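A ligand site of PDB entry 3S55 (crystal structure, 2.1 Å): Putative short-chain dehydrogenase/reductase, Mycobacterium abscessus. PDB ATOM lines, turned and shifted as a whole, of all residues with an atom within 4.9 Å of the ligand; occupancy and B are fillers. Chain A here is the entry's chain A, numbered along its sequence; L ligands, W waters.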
ATOM      1  N   GLY A  17     -15.448  17.632 -25.271  1.00  0.00           N
ATOM      2  CA  GLY A  17     -15.626  16.180 -25.225  1.00  0.00           C
ATOM      3  C   GLY A  17     -14.734  15.488 -26.256  1.00  0.00           C
ATOM      4  O   GLY A  17     -15.132  14.470 -26.835  1.00  0.00           O
ATOM      5  N   ALA A  19     -12.014  13.751 -25.974  1.00  0.00           N
ATOM      6  CA  ALA A  19     -11.164  12.622 -25.539  1.00  0.00           C
ATOM      7  C   ALA A  19     -11.406  11.283 -26.230  1.00  0.00           C
ATOM      8  O   ALA A  19     -10.495  10.425 -26.262  1.00  0.00           O
ATOM      9  CB  ALA A  19     -11.225  12.438 -24.040  1.00  0.00           C
ATOM     10  N   ARG A  20     -12.618  11.071 -26.744  1.00  0.00           N
ATOM     11  CA  ARG A  20     -12.975   9.826 -27.433  1.00  0.00           C
ATOM     12  C   ARG A  20     -14.183   9.981 -28.374  1.00  0.00           C
ATOM     13  O   ARG A  20     -14.717  11.098 -28.546  1.00  0.00           O
ATOM     14  CB  ARG A  20     -13.253   8.717 -26.393  1.00  0.00           C
ATOM     15  CG  ARG A  20     -14.561   8.894 -25.652  1.00  0.00           C
ATOM     16  CD  ARG A  20     -14.770   7.912 -24.477  1.00  0.00           C
ATOM     17  NE  ARG A  20     -16.158   8.008 -24.014  1.00  0.00           N
ATOM     18  CZ  ARG A  20     -16.648   7.439 -22.918  1.00  0.00           C
ATOM     19  NH1 ARG A  20     -17.926   7.611 -22.607  1.00  0.00           N
ATOM     20  NH2 ARG A  20     -15.876   6.687 -22.121  1.00  0.00           N
ATOM     21  N   GLY A  21     -14.613   8.875 -28.965  1.00  0.00           N
ATOM     22  CA  GLY A  21     -15.880   8.826 -29.713  1.00  0.00           C
ATOM     23  C   GLY A  21     -15.921   9.876 -30.801  1.00  0.00           C
ATOM     24  O   GLY A  21     -14.915  10.104 -31.464  1.00  0.00           O
ATOM     25  N   MET A  22     -17.072  10.533 -30.965  1.00  0.00           N
ATOM     26  CA  MET A  22     -17.265  11.518 -32.045  1.00  0.00           C
ATOM     27  C   MET A  22     -16.331  12.722 -31.960  1.00  0.00           C
ATOM     28  O   MET A  22     -15.909  13.264 -33.000  1.00  0.00           O
ATOM     29  CB  MET A  22     -18.733  11.987 -32.126  1.00  0.00           C
ATOM     30  CG  MET A  22     -19.582  11.044 -32.948  1.00  0.00           C
ATOM     31  SD  MET A  22     -21.291  11.490 -33.271  1.00  0.00           S
ATOM     32  CE  MET A  22     -22.094  10.949 -31.759  1.00  0.00           C
ATOM     33  N   GLY A  23     -16.037  13.153 -30.733  1.00  0.00           N
ATOM     34  CA  GLY A  23     -15.200  14.333 -30.504  1.00  0.00           C
ATOM     35  C   GLY A  23     -13.795  14.090 -31.042  1.00  0.00           C
ATOM     36  O   GLY A  23     -13.224  14.958 -31.703  1.00  0.00           O
ATOM     37  N   ASP A  41     -11.830  17.881 -22.290  1.00  0.00           N
ATOM     38  CA  ASP A  41     -12.699  16.852 -21.834  1.00  0.00           C
ATOM     39  C   ASP A  41     -12.620  16.815 -20.330  1.00  0.00           C
ATOM     40  O   ASP A  41     -11.594  17.156 -19.731  1.00  0.00           O
ATOM     41  CB  ASP A  41     -12.254  15.518 -22.404  1.00  0.00           C
ATOM     42  CG  ASP A  41     -13.362  14.494 -22.432  1.00  0.00           C
ATOM     43  OD1 ASP A  41     -13.791  14.123 -23.543  1.00  0.00           O
ATOM     44  OD2 ASP A  41     -13.796  14.045 -21.357  1.00  0.00           O
ATOM     45  N   ARG A  42     -13.723  16.402 -19.725  1.00  0.00           N
ATOM     46  CA  ARG A  42     -13.835  16.327 -18.289  1.00  0.00           C
ATOM     47  C   ARG A  42     -12.923  15.231 -17.708  1.00  0.00           C
ATOM     48  O   ARG A  42     -12.476  15.363 -16.573  1.00  0.00           O
ATOM     49  CB  ARG A  42     -15.290  16.052 -17.962  1.00  0.00           C
ATOM     50  CG  ARG A  42     -15.667  16.045 -16.523  1.00  0.00           C
ATOM     51  CD  ARG A  42     -16.902  15.180 -16.366  1.00  0.00           C
ATOM     52  NE  ARG A  42     -17.090  14.854 -14.965  1.00  0.00           N
ATOM     53  CZ  ARG A  42     -18.235  14.917 -14.323  1.00  0.00           C
ATOM     54  NH1 ARG A  42     -18.255  14.619 -13.027  1.00  0.00           N
ATOM     55  NH2 ARG A  42     -19.352  15.269 -14.966  1.00  0.00           N
ATOM     56  N   CYS A  43     -12.689  14.169 -18.477  1.00  0.00           N
ATOM     57  CA  CYS A  43     -11.773  13.068 -18.063  1.00  0.00           C
ATOM     58  C   CYS A  43     -12.074  12.467 -16.683  1.00  0.00           C
ATOM     59  O   CYS A  43     -11.168  12.173 -15.913  1.00  0.00           O
ATOM     60  CB  CYS A  43     -10.304  13.525 -18.103  1.00  0.00           C
ATOM     61  SG  CYS A  43      -9.814  14.126 -19.713  1.00  0.00           S
ATOM     62  N   TYR A  51     -22.449   4.644 -17.451  1.00  0.00           N
ATOM     63  CA  TYR A  51     -21.320   4.119 -18.218  1.00  0.00           C
ATOM     64  C   TYR A  51     -20.025   4.952 -17.957  1.00  0.00           C
ATOM     65  O   TYR A  51     -20.114   6.132 -17.604  1.00  0.00           O
ATOM     66  CB  TYR A  51     -21.678   4.059 -19.715  1.00  0.00           C
ATOM     67  CG  TYR A  51     -22.079   5.404 -20.282  1.00  0.00           C
ATOM     68  CD1 TYR A  51     -21.112   6.259 -20.820  1.00  0.00           C
ATOM     69  CD2 TYR A  51     -23.434   5.827 -20.303  1.00  0.00           C
ATOM     70  CE1 TYR A  51     -21.464   7.494 -21.347  1.00  0.00           C
ATOM     71  CE2 TYR A  51     -23.798   7.080 -20.826  1.00  0.00           C
ATOM     72  CZ  TYR A  51     -22.798   7.901 -21.355  1.00  0.00           C
ATOM     73  OH  TYR A  51     -23.068   9.129 -21.882  1.00  0.00           O
ATOM     74  N   LEU A  53     -17.066   7.454 -18.394  1.00  0.00           N
ATOM     75  CA  LEU A  53     -16.689   8.576 -19.249  1.00  0.00           C
ATOM     76  C   LEU A  53     -15.208   8.451 -19.643  1.00  0.00           C
ATOM     77  O   LEU A  53     -14.526   7.480 -19.281  1.00  0.00           O
ATOM     78  CB  LEU A  53     -17.014   9.911 -18.562  1.00  0.00           C
ATOM     79  CG  LEU A  53     -18.488  10.121 -18.142  1.00  0.00           C
ATOM     80  CD1 LEU A  53     -18.738  11.549 -17.682  1.00  0.00           C
ATOM     81  CD2 LEU A  53     -19.438   9.783 -19.269  1.00  0.00           C
ATOM     82  N   ALA A  54     -14.701   9.410 -20.413  1.00  0.00           N
ATOM     83  CA  ALA A  54     -13.304   9.389 -20.848  1.00  0.00           C
ATOM     84  C   ALA A  54     -12.310   9.524 -19.684  1.00  0.00           C
ATOM     85  O   ALA A  54     -12.656   9.988 -18.591  1.00  0.00           O
ATOM     86  CB  ALA A  54     -13.068  10.471 -21.882  1.00  0.00           C
ATOM     87  N   VAL A  78     -11.331  19.809 -18.753  1.00  0.00           N
ATOM     88  CA  VAL A  78     -12.329  20.872 -18.558  1.00  0.00           C
ATOM     89  C   VAL A  78     -13.741  20.294 -18.504  1.00  0.00           C
ATOM     90  O   VAL A  78     -14.126  19.495 -19.369  1.00  0.00           O
ATOM     91  CB  VAL A  78     -12.259  21.959 -19.671  1.00  0.00           C
ATOM     92  CG1 VAL A  78     -13.257  23.109 -19.421  1.00  0.00           C
ATOM     93  CG2 VAL A  78     -10.826  22.533 -19.807  1.00  0.00           C
ATOM     94  N   ASP A  79     -14.486  20.684 -17.478  1.00  0.00           N
ATOM     95  CA  ASP A  79     -15.917  20.435 -17.359  1.00  0.00           C
ATOM     96  C   ASP A  79     -16.666  21.612 -18.005  1.00  0.00           C
ATOM     97  O   ASP A  79     -16.599  22.720 -17.506  1.00  0.00           O
ATOM     98  CB  ASP A  79     -16.290  20.322 -15.855  1.00  0.00           C
ATOM     99  CG  ASP A  79     -17.778  20.026 -15.587  1.00  0.00           C
ATOM    100  OD1 ASP A  79     -18.590  19.830 -16.541  1.00  0.00           O
ATOM    101  OD2 ASP A  79     -18.142  20.009 -14.379  1.00  0.00           O
ATOM    102  N   VAL A  80     -17.379  21.348 -19.098  1.00  0.00           N
ATOM    103  CA  VAL A  80     -18.147  22.391 -19.837  1.00  0.00           C
ATOM    104  C   VAL A  80     -19.231  23.093 -19.001  1.00  0.00           C
ATOM    105  O   VAL A  80     -19.644  24.214 -19.340  1.00  0.00           O
ATOM    106  CB  VAL A  80     -18.772  21.857 -21.142  1.00  0.00           C
ATOM    107  CG1 VAL A  80     -17.668  21.410 -22.110  1.00  0.00           C
ATOM    108  CG2 VAL A  80     -19.770  20.718 -20.859  1.00  0.00           C
ATOM    109  N   LYS A  81     -19.688  22.448 -17.921  1.00  0.00           N
ATOM    110  CA  LYS A  81     -20.563  23.117 -16.943  1.00  0.00           C
ATOM    111  C   LYS A  81     -19.869  24.333 -16.306  1.00  0.00           C
ATOM    112  O   LYS A  81     -20.554  25.296 -15.888  1.00  0.00           O
ATOM    113  CB  LYS A  81     -21.067  22.161 -15.822  1.00  0.00           C
ATOM    114  CG  LYS A  81     -21.873  20.930 -16.318  1.00  0.00           C
ATOM    115  CD  LYS A  81     -22.677  20.260 -15.193  1.00  0.00           C
ATOM    116  CE  LYS A  81     -21.788  19.715 -14.035  1.00  0.00           C
ATOM    117  NZ  LYS A  81     -20.608  18.983 -14.603  1.00  0.00           N
ATOM    118  N   ASN A 106     -19.370  19.319 -28.556  1.00  0.00           N
ATOM    119  CA  ASN A 106     -19.642  17.901 -28.637  1.00  0.00           C
ATOM    120  C   ASN A 106     -19.769  17.194 -27.281  1.00  0.00           C
ATOM    121  O   ASN A 106     -20.414  16.157 -27.192  1.00  0.00           O
ATOM    122  CB  ASN A 106     -18.551  17.228 -29.495  1.00  0.00           C
ATOM    123  CG  ASN A 106     -18.518  15.710 -29.348  1.00  0.00           C
ATOM    124  OD1 ASN A 106     -19.222  14.994 -30.064  1.00  0.00           O
ATOM    125  ND2 ASN A 106     -17.704  15.222 -28.415  1.00  0.00           N
ATOM    126  N   ALA A 107     -19.161  17.771 -26.245  1.00  0.00           N
ATOM    127  CA  ALA A 107     -19.248  17.213 -24.894  1.00  0.00           C
ATOM    128  C   ALA A 107     -20.695  16.883 -24.526  1.00  0.00           C
ATOM    129  O   ALA A 107     -21.579  17.711 -24.647  1.00  0.00           O
ATOM    130  CB  ALA A 107     -18.691  18.238 -23.880  1.00  0.00           C
ATOM    131  N   GLY A 108     -20.944  15.673 -24.072  1.00  0.00           N
ATOM    132  CA  GLY A 108     -22.317  15.348 -23.679  1.00  0.00           C
ATOM    133  C   GLY A 108     -22.463  13.988 -23.045  1.00  0.00           C
ATOM    134  O   GLY A 108     -21.571  13.149 -23.162  1.00  0.00           O
ATOM    135  N   ILE A 109     -23.596  13.770 -22.378  1.00  0.00           N
ATOM    136  CA  ILE A 109     -23.862  12.519 -21.670  1.00  0.00           C
ATOM    137  C   ILE A 109     -25.284  12.052 -21.939  1.00  0.00           C
ATOM    138  O   ILE A 109     -26.165  12.855 -22.328  1.00  0.00           O
ATOM    139  CB  ILE A 109     -23.636  12.645 -20.108  1.00  0.00           C
ATOM    140  CG1 ILE A 109     -24.370  13.879 -19.548  1.00  0.00           C
ATOM    141  CG2 ILE A 109     -22.140  12.683 -19.776  1.00  0.00           C
ATOM    142  CD1 ILE A 109     -24.488  13.879 -18.052  1.00  0.00           C
ATOM    143  N   GLU A 125     -27.308  17.166 -14.074  1.00  0.00           N
ATOM    144  CA  GLU A 125     -26.057  16.892 -14.773  1.00  0.00           C
ATOM    145  C   GLU A 125     -26.223  16.862 -16.296  1.00  0.00           C
ATOM    146  O   GLU A 125     -25.365  17.342 -17.039  1.00  0.00           O
ATOM    147  CB  GLU A 125     -25.462  15.585 -14.247  1.00  0.00           C
ATOM    148  CG  GLU A 125     -24.091  15.196 -14.866  1.00  0.00           C
ATOM    149  CD  GLU A 125     -22.993  16.217 -14.643  1.00  0.00           C
ATOM    150  OE1 GLU A 125     -22.823  16.701 -13.494  1.00  0.00           O
ATOM    151  OE2 GLU A 125     -22.273  16.519 -15.624  1.00  0.00           O
ATOM    152  N   THR A 129     -24.527  19.542 -18.412  1.00  0.00           N
ATOM    153  CA  THR A 129     -23.497  19.203 -19.405  1.00  0.00           C
ATOM    154  C   THR A 129     -23.959  19.457 -20.842  1.00  0.00           C
ATOM    155  O   THR A 129     -23.271  20.142 -21.595  1.00  0.00           O
ATOM    156  CB  THR A 129     -23.033  17.734 -19.276  1.00  0.00           C
ATOM    157  OG1 THR A 129     -22.429  17.529 -18.002  1.00  0.00           O
ATOM    158  CG2 THR A 129     -22.000  17.356 -20.368  1.00  0.00           C
ATOM    159  N   ASN A 130     -25.108  18.902 -21.219  1.00  0.00           N
ATOM    160  CA  ASN A 130     -25.579  18.914 -22.617  1.00  0.00           C
ATOM    161  C   ASN A 130     -26.096  20.268 -23.104  1.00  0.00           C
ATOM    162  O   ASN A 130     -25.863  20.637 -24.233  1.00  0.00           O
ATOM    163  CB  ASN A 130     -26.685  17.862 -22.840  1.00  0.00           C
ATOM    164  CG  ASN A 130     -26.187  16.428 -22.727  1.00  0.00           C
ATOM    165  OD1 ASN A 130     -25.010  16.179 -22.504  1.00  0.00           O
ATOM    166  ND2 ASN A 130     -27.106  15.472 -22.915  1.00  0.00           N
ATOM    167  N   VAL A 156     -24.184  19.833 -31.142  1.00  0.00           N
ATOM    168  CA  VAL A 156     -24.575  18.451 -31.277  1.00  0.00           C
ATOM    169  C   VAL A 156     -25.865  18.161 -30.551  1.00  0.00           C
ATOM    170  O   VAL A 156     -25.925  18.156 -29.324  1.00  0.00           O
ATOM    171  CB  VAL A 156     -23.520  17.475 -30.769  1.00  0.00           C
ATOM    172  CG1 VAL A 156     -23.980  16.054 -31.081  1.00  0.00           C
ATOM    173  CG2 VAL A 156     -22.178  17.747 -31.453  1.00  0.00           C
ATOM    174  N   SER A 157     -26.916  17.942 -31.323  1.00  0.00           N
ATOM    175  CA  SER A 157     -28.182  17.592 -30.740  1.00  0.00           C
ATOM    176  C   SER A 157     -28.312  16.099 -30.891  1.00  0.00           C
ATOM    177  O   SER A 157     -27.368  15.358 -30.599  1.00  0.00           O
ATOM    178  CB  SER A 157     -29.333  18.362 -31.422  1.00  0.00           C
ATOM    179  OG  SER A 157     -30.602  17.921 -30.938  1.00  0.00           O
ATOM    180  N   SER A 158     -29.459  15.648 -31.361  1.00  0.00           N
ATOM    181  CA  SER A 158     -29.729  14.234 -31.515  1.00  0.00           C
ATOM    182  C   SER A 158     -31.011  14.074 -32.327  1.00  0.00           C
ATOM    183  O   SER A 158     -31.806  15.016 -32.476  1.00  0.00           O
ATOM    184  CB  SER A 158     -29.834  13.542 -30.140  1.00  0.00           C
ATOM    185  OG  SER A 158     -30.605  12.358 -30.206  1.00  0.00           O
ATOM    186  N   TYR A 171     -32.281  13.656 -21.110  1.00  0.00           N
ATOM    187  CA  TYR A 171     -31.550  13.709 -22.367  1.00  0.00           C
ATOM    188  C   TYR A 171     -32.328  14.483 -23.458  1.00  0.00           C
ATOM    189  O   TYR A 171     -31.794  15.447 -24.010  1.00  0.00           O
ATOM    190  CB  TYR A 171     -31.225  12.306 -22.816  1.00  0.00           C
ATOM    191  CG  TYR A 171     -30.293  12.258 -23.996  1.00  0.00           C
ATOM    192  CD1 TYR A 171     -28.926  12.473 -23.822  1.00  0.00           C
ATOM    193  CD2 TYR A 171     -30.760  11.977 -25.267  1.00  0.00           C
ATOM    194  CE1 TYR A 171     -28.043  12.418 -24.889  1.00  0.00           C
ATOM    195  CE2 TYR A 171     -29.889  11.909 -26.336  1.00  0.00           C
ATOM    196  CZ  TYR A 171     -28.532  12.146 -26.137  1.00  0.00           C
ATOM    197  OH  TYR A 171     -27.659  12.068 -27.205  1.00  0.00           O
ATOM    198  N   LYS A 175     -31.533  18.125 -25.546  1.00  0.00           N
ATOM    199  CA  LYS A 175     -31.234  18.110 -26.981  1.00  0.00           C
ATOM    200  C   LYS A 175     -32.256  18.929 -27.808  1.00  0.00           C
ATOM    201  O   LYS A 175     -31.920  19.442 -28.897  1.00  0.00           O
ATOM    202  CB  LYS A 175     -31.100  16.667 -27.499  1.00  0.00           C
ATOM    203  CG  LYS A 175     -29.937  15.835 -26.848  1.00  0.00           C
ATOM    204  CD  LYS A 175     -28.557  16.444 -27.160  1.00  0.00           C
ATOM    205  CE  LYS A 175     -27.423  15.524 -26.839  1.00  0.00           C
ATOM    206  NZ  LYS A 175     -26.102  16.123 -27.268  1.00  0.00           N
ATOM    207  N   PRO A 201     -27.294  13.432 -34.700  1.00  0.00           N
ATOM    208  CA  PRO A 201     -27.019  12.019 -35.059  1.00  0.00           C
ATOM    209  C   PRO A 201     -28.100  11.027 -34.579  1.00  0.00           C
ATOM    210  O   PRO A 201     -28.783  11.304 -33.568  1.00  0.00           O
ATOM    211  CB  PRO A 201     -25.660  11.729 -34.394  1.00  0.00           C
ATOM    212  CG  PRO A 201     -25.099  13.115 -33.983  1.00  0.00           C
ATOM    213  CD  PRO A 201     -26.292  14.003 -33.790  1.00  0.00           C
ATOM    214  N   GLY A 202     -28.271   9.920 -35.323  1.00  0.00           N
ATOM    215  CA  GLY A 202     -29.005   8.730 -34.868  1.00  0.00           C
ATOM    216  C   GLY A 202     -28.072   7.921 -33.991  1.00  0.00           C
ATOM    217  O   GLY A 202     -27.221   8.526 -33.305  1.00  0.00           O
ATOM    218  N   ASN A 203     -28.178   6.588 -33.999  1.00  0.00           N
ATOM    219  CA  ASN A 203     -27.331   5.775 -33.128  1.00  0.00           C
ATOM    220  C   ASN A 203     -25.908   5.646 -33.675  1.00  0.00           C
ATOM    221  O   ASN A 203     -25.664   5.134 -34.770  1.00  0.00           O
ATOM    222  CB  ASN A 203     -27.969   4.414 -32.816  1.00  0.00           C
ATOM    223  CG  ASN A 203     -29.396   4.542 -32.277  1.00  0.00           C
ATOM    224  OD1 ASN A 203     -30.344   4.175 -32.965  1.00  0.00           O
ATOM    225  ND2 ASN A 203     -29.555   5.069 -31.060  1.00  0.00           N
ATOM    226  N   ILE A 204     -24.961   6.142 -32.907  1.00  0.00           N
ATOM    227  CA  ILE A 204     -23.583   6.117 -33.354  1.00  0.00           C
ATOM    228  C   ILE A 204     -22.785   5.120 -32.501  1.00  0.00           C
ATOM    229  O   ILE A 204     -22.973   5.062 -31.282  1.00  0.00           O
ATOM    230  CB  ILE A 204     -22.968   7.522 -33.273  1.00  0.00           C
ATOM    231  CG1 ILE A 204     -23.905   8.571 -33.865  1.00  0.00           C
ATOM    232  CG2 ILE A 204     -21.579   7.576 -33.977  1.00  0.00           C
ATOM    233  CD1 ILE A 204     -24.278   8.346 -35.356  1.00  0.00           C
ATOM    234  N   THR A 206     -20.049   4.523 -30.435  1.00  0.00           N
ATOM    235  CA  THR A 206     -19.042   5.226 -29.649  1.00  0.00           C
ATOM    236  C   THR A 206     -19.143   4.596 -28.275  1.00  0.00           C
ATOM    237  O   THR A 206     -20.054   3.793 -28.039  1.00  0.00           O
ATOM    238  CB  THR A 206     -19.366   6.743 -29.504  1.00  0.00           C
ATOM    239  OG1 THR A 206     -20.455   6.924 -28.576  1.00  0.00           O
ATOM    240  CG2 THR A 206     -19.704   7.384 -30.843  1.00  0.00           C
ATOM    241  N   PRO A 207     -18.221   4.941 -27.345  1.00  0.00           N
ATOM    242  CA  PRO A 207     -18.360   4.353 -26.005  1.00  0.00           C
ATOM    243  C   PRO A 207     -19.585   4.815 -25.193  1.00  0.00           C
ATOM    244  O   PRO A 207     -19.857   4.230 -24.128  1.00  0.00           O
ATOM    245  CB  PRO A 207     -17.037   4.763 -25.313  1.00  0.00           C
ATOM    246  CG  PRO A 207     -16.094   5.049 -26.434  1.00  0.00           C
ATOM    247  CD  PRO A 207     -16.958   5.701 -27.475  1.00  0.00           C
ATOM    248  N   MET A 208     -20.318   5.818 -25.672  1.00  0.00           N
ATOM    249  CA  MET A 208     -21.635   6.193 -25.082  1.00  0.00           C
ATOM    250  C   MET A 208     -22.675   5.085 -25.264  1.00  0.00           C
ATOM    251  O   MET A 208     -23.491   4.818 -24.375  1.00  0.00           O
ATOM    252  CB  MET A 208     -22.168   7.536 -25.653  1.00  0.00           C
ATOM    253  CG  MET A 208     -23.554   7.958 -25.090  1.00  0.00           C
ATOM    254  SD  MET A 208     -24.411   9.382 -25.849  1.00  0.00           S
ATOM    255  CE  MET A 208     -23.648  10.718 -24.924  1.00  0.00           C
ATOM    256  N   THR A 209     -22.639   4.402 -26.402  1.00  0.00           N
ATOM    257  CA  THR A 209     -23.625   3.365 -26.676  1.00  0.00           C
ATOM    258  C   THR A 209     -23.048   1.957 -26.544  1.00  0.00           C
ATOM    259  O   THR A 209     -23.794   1.016 -26.237  1.00  0.00           O
ATOM    260  CB  THR A 209     -24.226   3.537 -28.086  1.00  0.00           C
ATOM    261  OG1 THR A 209     -23.154   3.586 -29.037  1.00  0.00           O
ATOM    262  CG2 THR A 209     -25.054   4.818 -28.151  1.00  0.00           C
HETATM  263  P1  LIG L   1     -18.717   9.619 -25.687  1.00  0.00           P
HETATM  264  O1  LIG L   1     -19.194   9.429 -24.272  1.00  0.00           O
HETATM  265  O2  LIG L   1     -17.752   8.598 -26.237  1.00  0.00           O
HETATM  266  O3  LIG L   1     -18.021  11.058 -25.814  1.00  0.00           O
HETATM  267  C1  LIG L   1     -18.501  12.149 -25.058  1.00  0.00           C
HETATM  268  C2  LIG L   1     -17.310  12.848 -24.415  1.00  0.00           C
HETATM  269  O4  LIG L   1     -17.768  13.993 -23.671  1.00  0.00           O
HETATM  270  C3  LIG L   1     -16.598  11.922 -23.420  1.00  0.00           C
HETATM  271  O5  LIG L   1     -15.190  11.874 -23.726  1.00  0.00           O
HETATM  272  C4  LIG L   1     -16.880  12.533 -22.063  1.00  0.00           C
HETATM  273  O6  LIG L   1     -15.827  12.396 -21.081  1.00  0.00           O
HETATM  274  C5  LIG L   1     -17.113  13.999 -22.411  1.00  0.00           C
HETATM  275  N1  LIG L   1     -17.880  14.732 -21.380  1.00  0.00           N
HETATM  276  C6  LIG L   1     -18.989  14.323 -20.725  1.00  0.00           C
HETATM  277  N2  LIG L   1     -19.362  15.291 -19.856  1.00  0.00           N
HETATM  278  C7  LIG L   1     -18.489  16.301 -19.981  1.00  0.00           C
HETATM  279  C8  LIG L   1     -18.380  17.549 -19.369  1.00  0.00           C
HETATM  280  N3  LIG L   1     -19.244  17.963 -18.419  1.00  0.00           N
HETATM  281  N4  LIG L   1     -17.358  18.346 -19.752  1.00  0.00           N
HETATM  282  C9  LIG L   1     -16.467  17.968 -20.690  1.00  0.00           C
HETATM  283  N5  LIG L   1     -16.544  16.777 -21.297  1.00  0.00           N
HETATM  284  C10 LIG L   1     -17.564  15.946 -20.955  1.00  0.00           C
HETATM  285  O7  LIG L   1     -20.051   9.718 -26.577  1.00  0.00           O
HETATM  286  P2  LIG L   1     -20.221  10.344 -28.048  1.00  0.00           P
HETATM  287  O8  LIG L   1     -21.122   9.381 -28.765  1.00  0.00           O
HETATM  288  O9  LIG L   1     -18.901  10.687 -28.697  1.00  0.00           O
HETATM  289  O10 LIG L   1     -21.057  11.673 -27.694  1.00  0.00           O
HETATM  290  C11 LIG L   1     -20.797  12.957 -28.251  1.00  0.00           C
HETATM  291  C12 LIG L   1     -22.098  13.782 -28.419  1.00  0.00           C
HETATM  292  O11 LIG L   1     -22.939  13.198 -29.433  1.00  0.00           O
HETATM  293  C13 LIG L   1     -22.943  13.934 -27.158  1.00  0.00           C
HETATM  294  O12 LIG L   1     -23.486  15.276 -27.074  1.00  0.00           O
HETATM  295  C14 LIG L   1     -24.103  13.014 -27.387  1.00  0.00           C
HETATM  296  O13 LIG L   1     -25.265  13.439 -26.652  1.00  0.00           O
HETATM  297  C15 LIG L   1     -24.261  13.107 -28.915  1.00  0.00           C
HETATM  298  N6  LIG L   1     -25.002  12.009 -29.511  1.00  0.00           N
HETATM  299  C16 LIG L   1     -24.503  10.752 -29.479  1.00  0.00           C
HETATM  300  C17 LIG L   1     -25.228   9.699 -30.059  1.00  0.00           C
HETATM  301  C18 LIG L   1     -24.719   8.270 -30.023  1.00  0.00           C
HETATM  302  O14 LIG L   1     -25.401   7.396 -30.522  1.00  0.00           O
HETATM  303  N7  LIG L   1     -23.547   7.973 -29.434  1.00  0.00           N
HETATM  304  C19 LIG L   1     -26.464   9.995 -30.657  1.00  0.00           C
HETATM  305  C20 LIG L   1     -26.952  11.306 -30.682  1.00  0.00           C
HETATM  306  C21 LIG L   1     -26.179  12.305 -30.109  1.00  0.00           C
HETATM  307  O   HOH W   1     -29.244   9.564 -28.678  1.00  0.00           O
HETATM  308  O   HOH W   2     -17.121  12.484 -28.145  1.00  0.00           O
HETATM  309  O   HOH W   3     -27.532   6.660 -29.363  1.00  0.00           O
HETATM  310  O   HOH W   4     -23.030  18.148 -26.913  1.00  0.00           O
HETATM  311  O   HOH W   5     -21.074  10.510 -22.554  1.00  0.00           O
HETATM  312  O   HOH W   6     -20.581  15.005 -17.074  1.00  0.00           O
HETATM  313  O   HOH W   7     -29.924   9.512 -31.023  1.00  0.00           O
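N of Ile 204 sits at hydrogen-bond distance from O14 of the ligand (2.7 Å).
OD2 of Asp 41 is in hydrogen-bond range of O6 of the ligand, 2.6 Å away.
The backbone NH of Met 22 lies within hydrogen-bond range of an oxygen (O9) of the ligand (2.9 Å).
OG1 of Thr 206 sits at hydrogen-bond distance from O8 of the ligand (2.6 Å).
An oxygen (O12) of the ligand sits close to the backbone carbonyl oxygen of Asn 106, at 3.2 Å.
N4 of the ligand lies within hydrogen-bond range of N of Val 80 (3.1 Å).
NZ of Lys 175 sits at hydrogen-bond distance from O12 of the ligand (2.8 Å).
A nitrogen (N7) of the ligand sits at hydrogen-bond distance from the backbone carbonyl oxygen (O) of Ile 204 (3.5 Å).
NH1 of Arg 20 lies within salt-bridge range of O1 of the ligand, 2.8 Å away.
The side-chain carboxylate of Asp 79 lies within hydrogen-bond range of a nitrogen (N3) of the ligand.
A nitrogen (N3) of the ligand lies within hydrogen-bond range of the side-chain hydroxyl (OG1) of Thr 129 (3.2 Å).
The backbone NH (N) of Ala 54 lies within hydrogen-bond range of an oxygen (O6) of the ligand, 3.3 Å away.
The side-chain hydroxyl (OH) of Tyr 171 sits at hydrogen-bond distance from an oxygen (O13) of the ligand, 2.8 Å away.
The backbone NH of Arg 42 sits at hydrogen-bond distance from a nitrogen (N5) of the ligand (3.3 Å).
The side-chain amino group (NZ) of Lys 175 sits at hydrogen-bond distance from the backbone carbonyl oxygen (O) of Val 156 (2.9 Å).
O of Leu 53 lies close to NH2 of Arg 20 (3.2 Å).
The backbone carbonyl oxygen of Asp 41 sits at hydrogen-bond distance from the backbone NH of Val 78.
OD2 of Asp 41 sits at hydrogen-bond distance from N of Cys 43.
O of Thr 206 lies within hydrogen-bond range of OG1 of Thr 209, 3.3 Å away.
O of Lys 175 sits at hydrogen-bond distance from OG of Ser 157, at 2.9 Å.
The backbone NH (N) of Arg 42 is in hydrogen-bond range of the backbone carbonyl oxygen (O) of Val 78 (3.1 Å).
The side-chain amino group (NZ) of Lys 81 is in salt-bridge range of the side-chain carboxylate (OD2) of Asp 79 (2.7 Å).
The backbone carbonyl oxygen of Val 78 lies close to a nitrogen (N4) of the ligand.
Residues that only touch the ligand: Gly 202 (3.1 Å), Met 208 (3.2 Å), Pro 207 (3.2 Å), Ser 157 (3.3 Å), Pro 201 (3.4 Å), Gly 17 (3.4 Å), Val 156 (3.5 Å), Thr 209 (3.5 Å), Gly 108 (3.6 Å), Asn 203 (3.6 Å), Ala 107 (3.7 Å), Ile 109 (3.7 Å), Ser 158 (3.7 Å), Gly 21 (3.7 Å) and Leu 53 (3.7 Å).
Hydrophobic or aromatic side chains that line the ligand: Met 22, Leu 53, Ala 54, Val 80, Ala 107, Ile 109, Val 156, Tyr 171, Pro 201, Ile 204, Pro 207 and Met 208.
29 residues have an atom within 4 Å of the ligand: Gly 17, Arg 20, Gly 21, Met 22, Asp 41, Arg 42, Leu 53, Ala 54, Val 78, Asp 79, Val 80, Asn 106, Ala 107, Gly 108, Ile 109, Thr 129, Val 156, Ser 157, Ser 158, Tyr 171, Lys 175, Pro 201, Gly 202, Asn 203, Ile 204, Thr 206, Pro 207, Met 208 and Thr 209.
Water W3 lies within hydrogen-bond range of O14 of the ligand (2.5 Å) and ND2 of Asn 203 (3.1 Å).
Water W5 lies within hydrogen-bond range of OH of Tyr 51, O of Gly 108 and O1 of the ligand.
Water W4 lies within hydrogen-bond range of the backbone carbonyl oxygen of Ala 107 (2.7 Å), an oxygen (O12) of the ligand (2.9 Å) and the backbone carbonyl oxygen of Asn 106 (3.3 Å).
Water W6 lies within hydrogen-bond range of NH2 of Arg 42 (2.5 Å), OE2 of Glu 125 (2.7 Å), N2 of the ligand (3.1 Å) and OG1 of Thr 129 (3.3 Å).
Water W1 bridges the side-chain hydroxyl (OH) of Tyr 171 (3.3 Å) and the side-chain hydroxyl (OG) of Ser 158 (3.5 Å).
Water W7 lies within hydrogen-bond range of the side-chain hydroxyl (OG) of Ser 158 (3.0 Å) and the backbone carbonyl oxygen (O) of Pro 201 (3.3 Å).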
